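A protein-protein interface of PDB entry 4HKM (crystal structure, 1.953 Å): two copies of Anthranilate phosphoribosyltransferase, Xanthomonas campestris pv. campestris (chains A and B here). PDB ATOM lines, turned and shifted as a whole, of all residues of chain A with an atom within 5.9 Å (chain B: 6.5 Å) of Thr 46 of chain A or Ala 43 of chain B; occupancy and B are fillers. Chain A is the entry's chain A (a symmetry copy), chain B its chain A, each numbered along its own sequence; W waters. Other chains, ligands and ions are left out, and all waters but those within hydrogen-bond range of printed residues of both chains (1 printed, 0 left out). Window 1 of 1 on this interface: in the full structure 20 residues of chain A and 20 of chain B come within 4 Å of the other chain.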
ATOM      1  N   THR A  13      25.540  15.631 -30.548  1.00  0.00           N
ATOM      2  CA  THR A  13      24.532  16.340 -29.757  1.00  0.00           C
ATOM      3  C   THR A  13      24.411  15.763 -28.354  1.00  0.00           C
ATOM      4  O   THR A  13      24.148  16.501 -27.392  1.00  0.00           O
ATOM      5  CB  THR A  13      23.139  16.324 -30.416  1.00  0.00           C
ATOM      6  OG1 THR A  13      22.595  15.001 -30.340  1.00  0.00           O
ATOM      7  CG2 THR A  13      23.215  16.773 -31.869  1.00  0.00           C
ATOM      8  N   ALA A  39      13.622   7.071 -37.275  1.00  0.00           N
ATOM      9  CA  ALA A  39      14.102   7.046 -35.885  1.00  0.00           C
ATOM     10  C   ALA A  39      15.435   7.775 -35.696  1.00  0.00           C
ATOM     11  O   ALA A  39      15.700   8.375 -34.628  1.00  0.00           O
ATOM     12  CB  ALA A  39      14.197   5.602 -35.370  1.00  0.00           C
ATOM     13  N   VAL A  41      16.434  10.298 -37.653  1.00  0.00           N
ATOM     14  CA  VAL A  41      16.119  11.711 -37.811  1.00  0.00           C
ATOM     15  C   VAL A  41      15.491  12.293 -36.552  1.00  0.00           C
ATOM     16  O   VAL A  41      15.877  13.378 -36.121  1.00  0.00           O
ATOM     17  CB  VAL A  41      15.201  11.976 -39.008  1.00  0.00           C
ATOM     18  CG1 VAL A  41      14.801  13.481 -39.044  1.00  0.00           C
ATOM     19  CG2 VAL A  41      15.917  11.577 -40.280  1.00  0.00           C
ATOM     20  N   SER A  42      14.543  11.581 -35.947  1.00  0.00           N
ATOM     21  CA  SER A  42      13.895  12.128 -34.752  1.00  0.00           C
ATOM     22  C   SER A  42      14.899  12.266 -33.591  1.00  0.00           C
ATOM     23  O   SER A  42      14.798  13.187 -32.760  1.00  0.00           O
ATOM     24  CB  SER A  42      12.676  11.292 -34.349  1.00  0.00           C
ATOM     25  OG  SER A  42      13.067   9.989 -33.940  1.00  0.00           O
ATOM     26  N   ALA A  43      15.867  11.351 -33.544  1.00  0.00           N
ATOM     27  CA  ALA A  43      16.909  11.389 -32.527  1.00  0.00           C
ATOM     28  C   ALA A  43      17.800  12.616 -32.721  1.00  0.00           C
ATOM     29  O   ALA A  43      18.053  13.342 -31.781  1.00  0.00           O
ATOM     30  CB  ALA A  43      17.740  10.094 -32.560  1.00  0.00           C
ATOM     31  N   ILE A  44      18.286  12.816 -33.936  1.00  0.00           N
ATOM     32  CA  ILE A  44      19.116  13.964 -34.250  1.00  0.00           C
ATOM     33  C   ILE A  44      18.353  15.284 -33.994  1.00  0.00           C
ATOM     34  O   ILE A  44      18.903  16.216 -33.371  1.00  0.00           O
ATOM     35  CB  ILE A  44      19.665  13.895 -35.695  1.00  0.00           C
ATOM     36  CG1 ILE A  44      20.712  12.772 -35.828  1.00  0.00           C
ATOM     37  CG2 ILE A  44      20.311  15.222 -36.087  1.00  0.00           C
ATOM     38  CD1 ILE A  44      20.943  12.292 -37.276  1.00  0.00           C
ATOM     39  N   LEU A  45      17.097  15.359 -34.434  1.00  0.00           N
ATOM     40  CA  LEU A  45      16.299  16.575 -34.212  1.00  0.00           C
ATOM     41  C   LEU A  45      16.095  16.881 -32.728  1.00  0.00           C
ATOM     42  O   LEU A  45      16.098  18.051 -32.312  1.00  0.00           O
ATOM     43  CB  LEU A  45      14.935  16.488 -34.929  1.00  0.00           C
ATOM     44  CG  LEU A  45      15.000  16.500 -36.456  1.00  0.00           C
ATOM     45  CD1 LEU A  45      13.610  16.392 -37.068  1.00  0.00           C
ATOM     46  CD2 LEU A  45      15.702  17.778 -36.936  1.00  0.00           C
ATOM     47  N   THR A  46      15.908  15.829 -31.935  1.00  0.00           N
ATOM     48  CA  THR A  46      15.743  16.001 -30.503  1.00  0.00           C
ATOM     49  C   THR A  46      17.055  16.466 -29.865  1.00  0.00           C
ATOM     50  O   THR A  46      17.063  17.430 -29.070  1.00  0.00           O
ATOM     51  CB  THR A  46      15.277  14.701 -29.832  1.00  0.00           C
ATOM     52  OG1 THR A  46      14.020  14.322 -30.389  1.00  0.00           O
ATOM     53  CG2 THR A  46      15.107  14.915 -28.343  1.00  0.00           C
ATOM     54  N   GLY A  47      18.162  15.812 -30.217  1.00  0.00           N
ATOM     55  CA  GLY A  47      19.459  16.232 -29.673  1.00  0.00           C
ATOM     56  C   GLY A  47      19.735  17.706 -29.954  1.00  0.00           C
ATOM     57  O   GLY A  47      20.208  18.463 -29.085  1.00  0.00           O
ATOM     58  N   LEU A  48      19.436  18.129 -31.176  1.00  0.00           N
ATOM     59  CA  LEU A  48      19.625  19.535 -31.560  1.00  0.00           C
ATOM     60  C   LEU A  48      18.744  20.490 -30.764  1.00  0.00           C
ATOM     61  O   LEU A  48      19.166  21.589 -30.383  1.00  0.00           O
ATOM     62  CB  LEU A  48      19.301  19.705 -33.048  1.00  0.00           C
ATOM     63  CG  LEU A  48      20.397  19.307 -34.026  1.00  0.00           C
ATOM     64  CD1 LEU A  48      19.798  19.288 -35.438  1.00  0.00           C
ATOM     65  CD2 LEU A  48      21.634  20.258 -33.906  1.00  0.00           C
ATOM     66  N   ARG A  49      17.515  20.065 -30.520  1.00  0.00           N
ATOM     67  CA  ARG A  49      16.511  20.876 -29.843  1.00  0.00           C
ATOM     68  C   ARG A  49      16.829  21.001 -28.360  1.00  0.00           C
ATOM     69  O   ARG A  49      16.704  22.089 -27.782  1.00  0.00           O
ATOM     70  CB  ARG A  49      15.133  20.241 -30.038  1.00  0.00           C
ATOM     71  CG  ARG A  49      13.981  21.010 -29.491  1.00  0.00           C
ATOM     72  CD  ARG A  49      13.688  22.255 -30.296  1.00  0.00           C
ATOM     73  NE  ARG A  49      13.023  23.217 -29.429  1.00  0.00           N
ATOM     74  CZ  ARG A  49      11.761  23.100 -29.029  1.00  0.00           C
ATOM     75  NH1 ARG A  49      11.242  24.011 -28.234  1.00  0.00           N
ATOM     76  NH2 ARG A  49      11.015  22.074 -29.434  1.00  0.00           N
ATOM     77  N   VAL A  50      17.237  19.899 -27.733  1.00  0.00           N
ATOM     78  CA  VAL A  50      17.612  19.958 -26.311  1.00  0.00           C
ATOM     79  C   VAL A  50      18.848  20.845 -26.087  1.00  0.00           C
ATOM     80  O   VAL A  50      18.879  21.706 -25.194  1.00  0.00           O
ATOM     81  CB  VAL A  50      17.859  18.546 -25.715  1.00  0.00           C
ATOM     82  CG1 VAL A  50      18.290  18.666 -24.234  1.00  0.00           C
ATOM     83  CG2 VAL A  50      16.601  17.706 -25.813  1.00  0.00           C
ATOM     84  N   LYS A  51      19.865  20.624 -26.904  1.00  0.00           N
ATOM     85  CA  LYS A  51      21.106  21.395 -26.882  1.00  0.00           C
ATOM     86  C   LYS A  51      20.846  22.870 -27.222  1.00  0.00           C
ATOM     87  O   LYS A  51      21.550  23.772 -26.763  1.00  0.00           O
ATOM     88  CB  LYS A  51      22.052  20.781 -27.930  1.00  0.00           C
ATOM     89  CG  LYS A  51      23.396  21.475 -28.106  1.00  0.00           C
ATOM     90  CD  LYS A  51      24.157  20.823 -29.262  1.00  0.00           C
ATOM     91  CE  LYS A  51      23.656  21.309 -30.622  1.00  0.00           C
ATOM     92  NZ  LYS A  51      23.933  22.775 -30.762  1.00  0.00           N
ATOM     93  N   MET A 174       6.530  13.400 -34.143  1.00  0.00           N
ATOM     94  CA  MET A 174       7.184  14.032 -32.981  1.00  0.00           C
ATOM     95  C   MET A 174       6.282  15.027 -32.292  1.00  0.00           C
ATOM     96  O   MET A 174       6.199  15.041 -31.069  1.00  0.00           O
ATOM     97  CB  MET A 174       8.467  14.727 -33.407  1.00  0.00           C
ATOM     98  CG  MET A 174       9.525  13.748 -33.808  1.00  0.00           C
ATOM     99  SD  MET A 174      11.089  14.679 -34.446  1.00  0.00           S
ATOM    100  CE  MET A 174      11.680  15.402 -32.673  1.00  0.00           C
ATOM    101  N   THR A 178      10.936  21.618 -34.038  1.00  0.00           N
ATOM    102  CA  THR A 178      12.307  21.185 -34.304  1.00  0.00           C
ATOM    103  C   THR A 178      12.934  22.232 -35.202  1.00  0.00           C
ATOM    104  O   THR A 178      12.297  23.226 -35.539  1.00  0.00           O
ATOM    105  CB  THR A 178      12.393  19.810 -35.040  1.00  0.00           C
ATOM    106  OG1 THR A 178      12.012  19.968 -36.412  1.00  0.00           O
ATOM    107  CG2 THR A 178      11.501  18.756 -34.384  1.00  0.00           C
ATOM    108  N   LEU B  10       8.558  13.674 -24.287  1.00  0.00           N
ATOM    109  CA  LEU B  10       9.561  14.270 -25.168  1.00  0.00           C
ATOM    110  C   LEU B  10       9.700  15.770 -24.894  1.00  0.00           C
ATOM    111  O   LEU B  10      10.819  16.288 -24.786  1.00  0.00           O
ATOM    112  CB  LEU B  10       9.230  14.025 -26.645  1.00  0.00           C
ATOM    113  CG  LEU B  10      10.152  14.720 -27.650  1.00  0.00           C
ATOM    114  CD1 LEU B  10      11.592  14.223 -27.454  1.00  0.00           C
ATOM    115  CD2 LEU B  10       9.685  14.484 -29.100  1.00  0.00           C
ATOM    116  N   THR B  13      11.792  16.577 -21.711  1.00  0.00           N
ATOM    117  CA  THR B  13      13.245  16.497 -21.878  1.00  0.00           C
ATOM    118  C   THR B  13      13.782  17.662 -22.698  1.00  0.00           C
ATOM    119  O   THR B  13      14.902  18.136 -22.455  1.00  0.00           O
ATOM    120  CB  THR B  13      13.697  15.181 -22.541  1.00  0.00           C
ATOM    121  OG1 THR B  13      13.312  15.191 -23.920  1.00  0.00           O
ATOM    122  CG2 THR B  13      13.086  13.976 -21.838  1.00  0.00           C
ATOM    123  N   ILE B  14      12.972  18.148 -23.639  1.00  0.00           N
ATOM    124  CA  ILE B  14      13.302  19.359 -24.409  1.00  0.00           C
ATOM    125  C   ILE B  14      13.429  20.606 -23.507  1.00  0.00           C
ATOM    126  O   ILE B  14      14.254  21.508 -23.751  1.00  0.00           O
ATOM    127  CB  ILE B  14      12.278  19.557 -25.561  1.00  0.00           C
ATOM    128  CG1 ILE B  14      12.577  18.536 -26.678  1.00  0.00           C
ATOM    129  CG2 ILE B  14      12.299  20.980 -26.100  1.00  0.00           C
ATOM    130  CD1 ILE B  14      11.522  18.503 -27.743  1.00  0.00           C
ATOM    131  N   ASP B  38       8.823   3.715 -33.143  1.00  0.00           N
ATOM    132  CA  ASP B  38      10.299   3.777 -33.075  1.00  0.00           C
ATOM    133  C   ASP B  38      10.808   5.227 -33.042  1.00  0.00           C
ATOM    134  O   ASP B  38      11.715   5.554 -32.256  1.00  0.00           O
ATOM    135  CB  ASP B  38      10.953   3.059 -34.248  1.00  0.00           C
ATOM    136  CG  ASP B  38      11.019   1.548 -34.061  1.00  0.00           C
ATOM    137  OD1 ASP B  38      10.496   1.050 -33.046  1.00  0.00           O
ATOM    138  OD2 ASP B  38      11.586   0.856 -34.943  1.00  0.00           O
ATOM    139  N   ALA B  39      10.248   6.094 -33.888  1.00  0.00           N
ATOM    140  CA  ALA B  39      10.732   7.482 -33.925  1.00  0.00           C
ATOM    141  C   ALA B  39      10.457   8.249 -32.628  1.00  0.00           C
ATOM    142  O   ALA B  39      11.243   9.136 -32.220  1.00  0.00           O
ATOM    143  CB  ALA B  39      10.145   8.229 -35.131  1.00  0.00           C
ATOM    144  N   MET B  40       9.340   7.936 -31.982  1.00  0.00           N
ATOM    145  CA  MET B  40       9.021   8.604 -30.725  1.00  0.00           C
ATOM    146  C   MET B  40       9.905   8.057 -29.598  1.00  0.00           C
ATOM    147  O   MET B  40      10.346   8.799 -28.717  1.00  0.00           O
ATOM    148  CB  MET B  40       7.542   8.471 -30.379  1.00  0.00           C
ATOM    149  CG  MET B  40       7.188   9.101 -29.038  1.00  0.00           C
ATOM    150  SD  MET B  40       7.458  11.060 -28.990  1.00  0.00           S
ATOM    151  CE  MET B  40       5.711  11.639 -29.695  1.00  0.00           C
ATOM    152  N   VAL B  41      10.189   6.762 -29.644  1.00  0.00           N
ATOM    153  CA  VAL B  41      11.093   6.181 -28.660  1.00  0.00           C
ATOM    154  C   VAL B  41      12.511   6.715 -28.810  1.00  0.00           C
ATOM    155  O   VAL B  41      13.140   7.067 -27.814  1.00  0.00           O
ATOM    156  CB  VAL B  41      11.116   4.650 -28.719  1.00  0.00           C
ATOM    157  CG1 VAL B  41      12.191   4.100 -27.735  1.00  0.00           C
ATOM    158  CG2 VAL B  41       9.743   4.119 -28.371  1.00  0.00           C
ATOM    159  N   SER B  42      13.014   6.798 -30.040  1.00  0.00           N
ATOM    160  CA  SER B  42      14.387   7.278 -30.216  1.00  0.00           C
ATOM    161  C   SER B  42      14.521   8.749 -29.779  1.00  0.00           C
ATOM    162  O   SER B  42      15.575   9.176 -29.272  1.00  0.00           O
ATOM    163  CB  SER B  42      14.868   7.069 -31.655  1.00  0.00           C
ATOM    164  OG  SER B  42      14.123   7.872 -32.560  1.00  0.00           O
ATOM    165  N   ALA B  43      13.449   9.516 -29.973  1.00  0.00           N
ATOM    166  CA  ALA B  43      13.422  10.914 -29.565  1.00  0.00           C
ATOM    167  C   ALA B  43      13.477  11.027 -28.041  1.00  0.00           C
ATOM    168  O   ALA B  43      14.269  11.779 -27.513  1.00  0.00           O
ATOM    169  CB  ALA B  43      12.169  11.613 -30.123  1.00  0.00           C
ATOM    170  N   ILE B  44      12.614  10.293 -27.355  1.00  0.00           N
ATOM    171  CA  ILE B  44      12.594  10.291 -25.905  1.00  0.00           C
ATOM    172  C   ILE B  44      13.945   9.803 -25.334  1.00  0.00           C
ATOM    173  O   ILE B  44      14.499  10.431 -24.408  1.00  0.00           O
ATOM    174  CB  ILE B  44      11.411   9.462 -25.350  1.00  0.00           C
ATOM    175  CG1 ILE B  44      10.071  10.170 -25.629  1.00  0.00           C
ATOM    176  CG2 ILE B  44      11.558   9.257 -23.844  1.00  0.00           C
ATOM    177  CD1 ILE B  44       8.842   9.239 -25.583  1.00  0.00           C
ATOM    178  N   LEU B  45      14.490   8.722 -25.893  1.00  0.00           N
ATOM    179  CA  LEU B  45      15.784   8.208 -25.417  1.00  0.00           C
ATOM    180  C   LEU B  45      16.918   9.218 -25.595  1.00  0.00           C
ATOM    181  O   LEU B  45      17.818   9.324 -24.745  1.00  0.00           O
ATOM    182  CB  LEU B  45      16.146   6.877 -26.108  1.00  0.00           C
ATOM    183  CG  LEU B  45      15.252   5.691 -25.746  1.00  0.00           C
ATOM    184  CD1 LEU B  45      15.675   4.433 -26.491  1.00  0.00           C
ATOM    185  CD2 LEU B  45      15.288   5.458 -24.230  1.00  0.00           C
ATOM    186  N   THR B  46      16.880   9.951 -26.706  1.00  0.00           N
ATOM    187  CA  THR B  46      17.885  10.967 -26.958  1.00  0.00           C
ATOM    188  C   THR B  46      17.726  12.132 -25.977  1.00  0.00           C
ATOM    189  O   THR B  46      18.718  12.584 -25.367  1.00  0.00           O
ATOM    190  CB  THR B  46      17.803  11.492 -28.398  1.00  0.00           C
ATOM    191  OG1 THR B  46      18.024  10.406 -29.296  1.00  0.00           O
ATOM    192  CG2 THR B  46      18.868  12.543 -28.632  1.00  0.00           C
ATOM    193  N   GLY B  47      16.493  12.609 -25.801  1.00  0.00           N
ATOM    194  CA  GLY B  47      16.264  13.699 -24.846  1.00  0.00           C
ATOM    195  C   GLY B  47      16.778  13.344 -23.455  1.00  0.00           C
ATOM    196  O   GLY B  47      17.417  14.160 -22.763  1.00  0.00           O
ATOM    197  N   LEU B  48      16.508  12.115 -23.032  1.00  0.00           N
ATOM    198  CA  LEU B  48      16.978  11.642 -21.724  1.00  0.00           C
ATOM    199  C   LEU B  48      18.498  11.590 -21.623  1.00  0.00           C
ATOM    200  O   LEU B  48      19.086  11.920 -20.586  1.00  0.00           O
ATOM    201  CB  LEU B  48      16.429  10.235 -21.462  1.00  0.00           C
ATOM    202  CG  LEU B  48      14.994  10.155 -20.959  1.00  0.00           C
ATOM    203  CD1 LEU B  48      14.544   8.690 -21.020  1.00  0.00           C
ATOM    204  CD2 LEU B  48      14.863  10.769 -19.526  1.00  0.00           C
ATOM    205  N   VAL B  50      20.774  13.269 -23.573  1.00  0.00           N
ATOM    206  CA  VAL B  50      21.386  14.608 -23.609  1.00  0.00           C
ATOM    207  C   VAL B  50      21.279  15.316 -22.248  1.00  0.00           C
ATOM    208  O   VAL B  50      22.254  15.879 -21.728  1.00  0.00           O
ATOM    209  CB  VAL B  50      20.772  15.499 -24.720  1.00  0.00           C
ATOM    210  CG1 VAL B  50      21.419  16.904 -24.688  1.00  0.00           C
ATOM    211  CG2 VAL B  50      20.991  14.870 -26.081  1.00  0.00           C
ATOM    212  N   MET B 174      19.857   3.325 -33.486  1.00  0.00           N
ATOM    213  CA  MET B 174      20.482   4.502 -32.852  1.00  0.00           C
ATOM    214  C   MET B 174      21.976   4.346 -32.709  1.00  0.00           C
ATOM    215  O   MET B 174      22.725   5.273 -32.998  1.00  0.00           O
ATOM    216  CB  MET B 174      19.870   4.757 -31.483  1.00  0.00           C
ATOM    217  CG  MET B 174      18.454   5.229 -31.585  1.00  0.00           C
ATOM    218  SD  MET B 174      17.689   5.428 -29.826  1.00  0.00           S
ATOM    219  CE  MET B 174      18.748   7.039 -29.281  1.00  0.00           C
HETATM  220  O   HOH W   1      15.413  23.093 -25.546  1.00  0.00           O
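The side-chain hydroxyl (OG) of Ser 42 of chain A is in hydrogen-bond range of the backbone carbonyl oxygen (O) of Ala 39 of chain B (2.6 Å). The side-chain hydroxyl (OG) of Ser 42 of chain B lies within hydrogen-bond range of the backbone carbonyl oxygen (O) of Ala 39 of chain A. The side-chain hydroxyl (OG) of Ser 42 of chain B sits at hydrogen-bond distance from the side-chain hydroxyl (OG) of Ser 42 of chain A (2.7 Å).
OG1 of Thr 13 of chain B sits at hydrogen-bond distance from O of Leu 10 of chain B (2.9 Å). OG of Ser 42 of chain B sits at hydrogen-bond distance from O of Asp 38 of chain B. O of Ala 39 of chain B sits at hydrogen-bond distance from OG of Ser 42 of chain B (3.2 Å). The backbone carbonyl oxygen of Ser 42 of chain B is in hydrogen-bond range of the side-chain hydroxyl of Thr 46 of chain B, at 2.7 Å. The backbone carbonyl oxygen (O) of Ala 39 of chain A lies within hydrogen-bond range of the side-chain hydroxyl (OG) of Ser 42 of chain A, at 3.2 Å. OG1 of Thr 46 of chain A sits at hydrogen-bond distance from O of Ser 42 of chain A.
Thr 13 of chain A touches Val 50 of chain B. Ala 39 of chain A touches Ala 39 of chain B. Thr 46 of chain B touches Ala 43 of chain A (OG1 to CB, 3.3 Å). Thr 46 of chain A touches Leu 10 of chain B. Thr 46 of chain A touches Gly 47 of chain B. Gly 47 of chain A touches Thr 46 of chain B. Arg 49 of chain A touches Ile 14 of chain B. Val 50 of chain A touches Thr 13 of chain B. Val 50 of chain A touches Ile 14 of chain B. Val 50 of chain B touches Val 50 of chain A (CG1 to CG1, 3.6 Å).
Of the printed residues of chain B, Thr 46 of chain A touches Leu 10, Ala 43 and Gly 47. Printed residues of chain B within 4 Å of Gly 47 of chain A: Thr 46. Leu 48 of chain A touches none of the printed residues of chain B. Of the printed residues of chain A, Ala 43 of chain B touches Thr 46 (3.3 Å). Of the printed residues of chain A, Gly 47 of chain B touches Thr 46. The nearest residue of chain B that does not touch Thr 46 of chain A is Thr 46 of chain B (4.3 Å). The nearest printed residue of chain A that does not touch Ala 43 of chain B is Ser 42 of chain A (4.01 Å).
Printed residues of chain A that touch a printed residue of chain B: Thr 13, Ala 39, Ser 42, Ala 43, Thr 46, Gly 47, Arg 49, Val 50 and Met 174. Hydrophobic or aromatic side chains of chain A that line the printed part of chain B: Ala 39, Ala 43 and Val 50. Of the 16 printed residues of chain B, 11 touch a printed residue of chain A. Hydrophobic or aromatic side chains of chain B within 4 Å of the printed part of chain A: Leu 10, Ile 14, Ala 39, Met 40, Ala 43 and Val 50. Along chain B the printed residues that touch a printed residue of chain A span positions 10 to 50. Among the printed residues, 16 pairs touch across the chains. Among the printed residues, no Asp or Glu carboxylate lies within 4 Å of a Lys or Arg side-chain nitrogen of the other chain.
Thr 13 of chain A touches Val 50 of chain B, and with the chains exchanged Val 50 of chain A touches Thr 13 of chain B. Ala 39 of chain B touches its own counterpart, Ala 39 of chain A. Ser 42 of chain B touches its own counterpart, Ser 42 of chain A. Ala 43 of chain A touches Thr 46 of chain B, and with the chains exchanged Thr 46 of chain A touches Ala 43 of chain B. Of the 16 pairs that touch across the chains among the printed residues, 11 have their exchanged pair printed and touching as well.
Water W1 lies within hydrogen-bond range of the backbone carbonyl oxygen (O) of Ile 14 of chain B and the backbone carbonyl oxygen (O) of Arg 49 of chain A.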
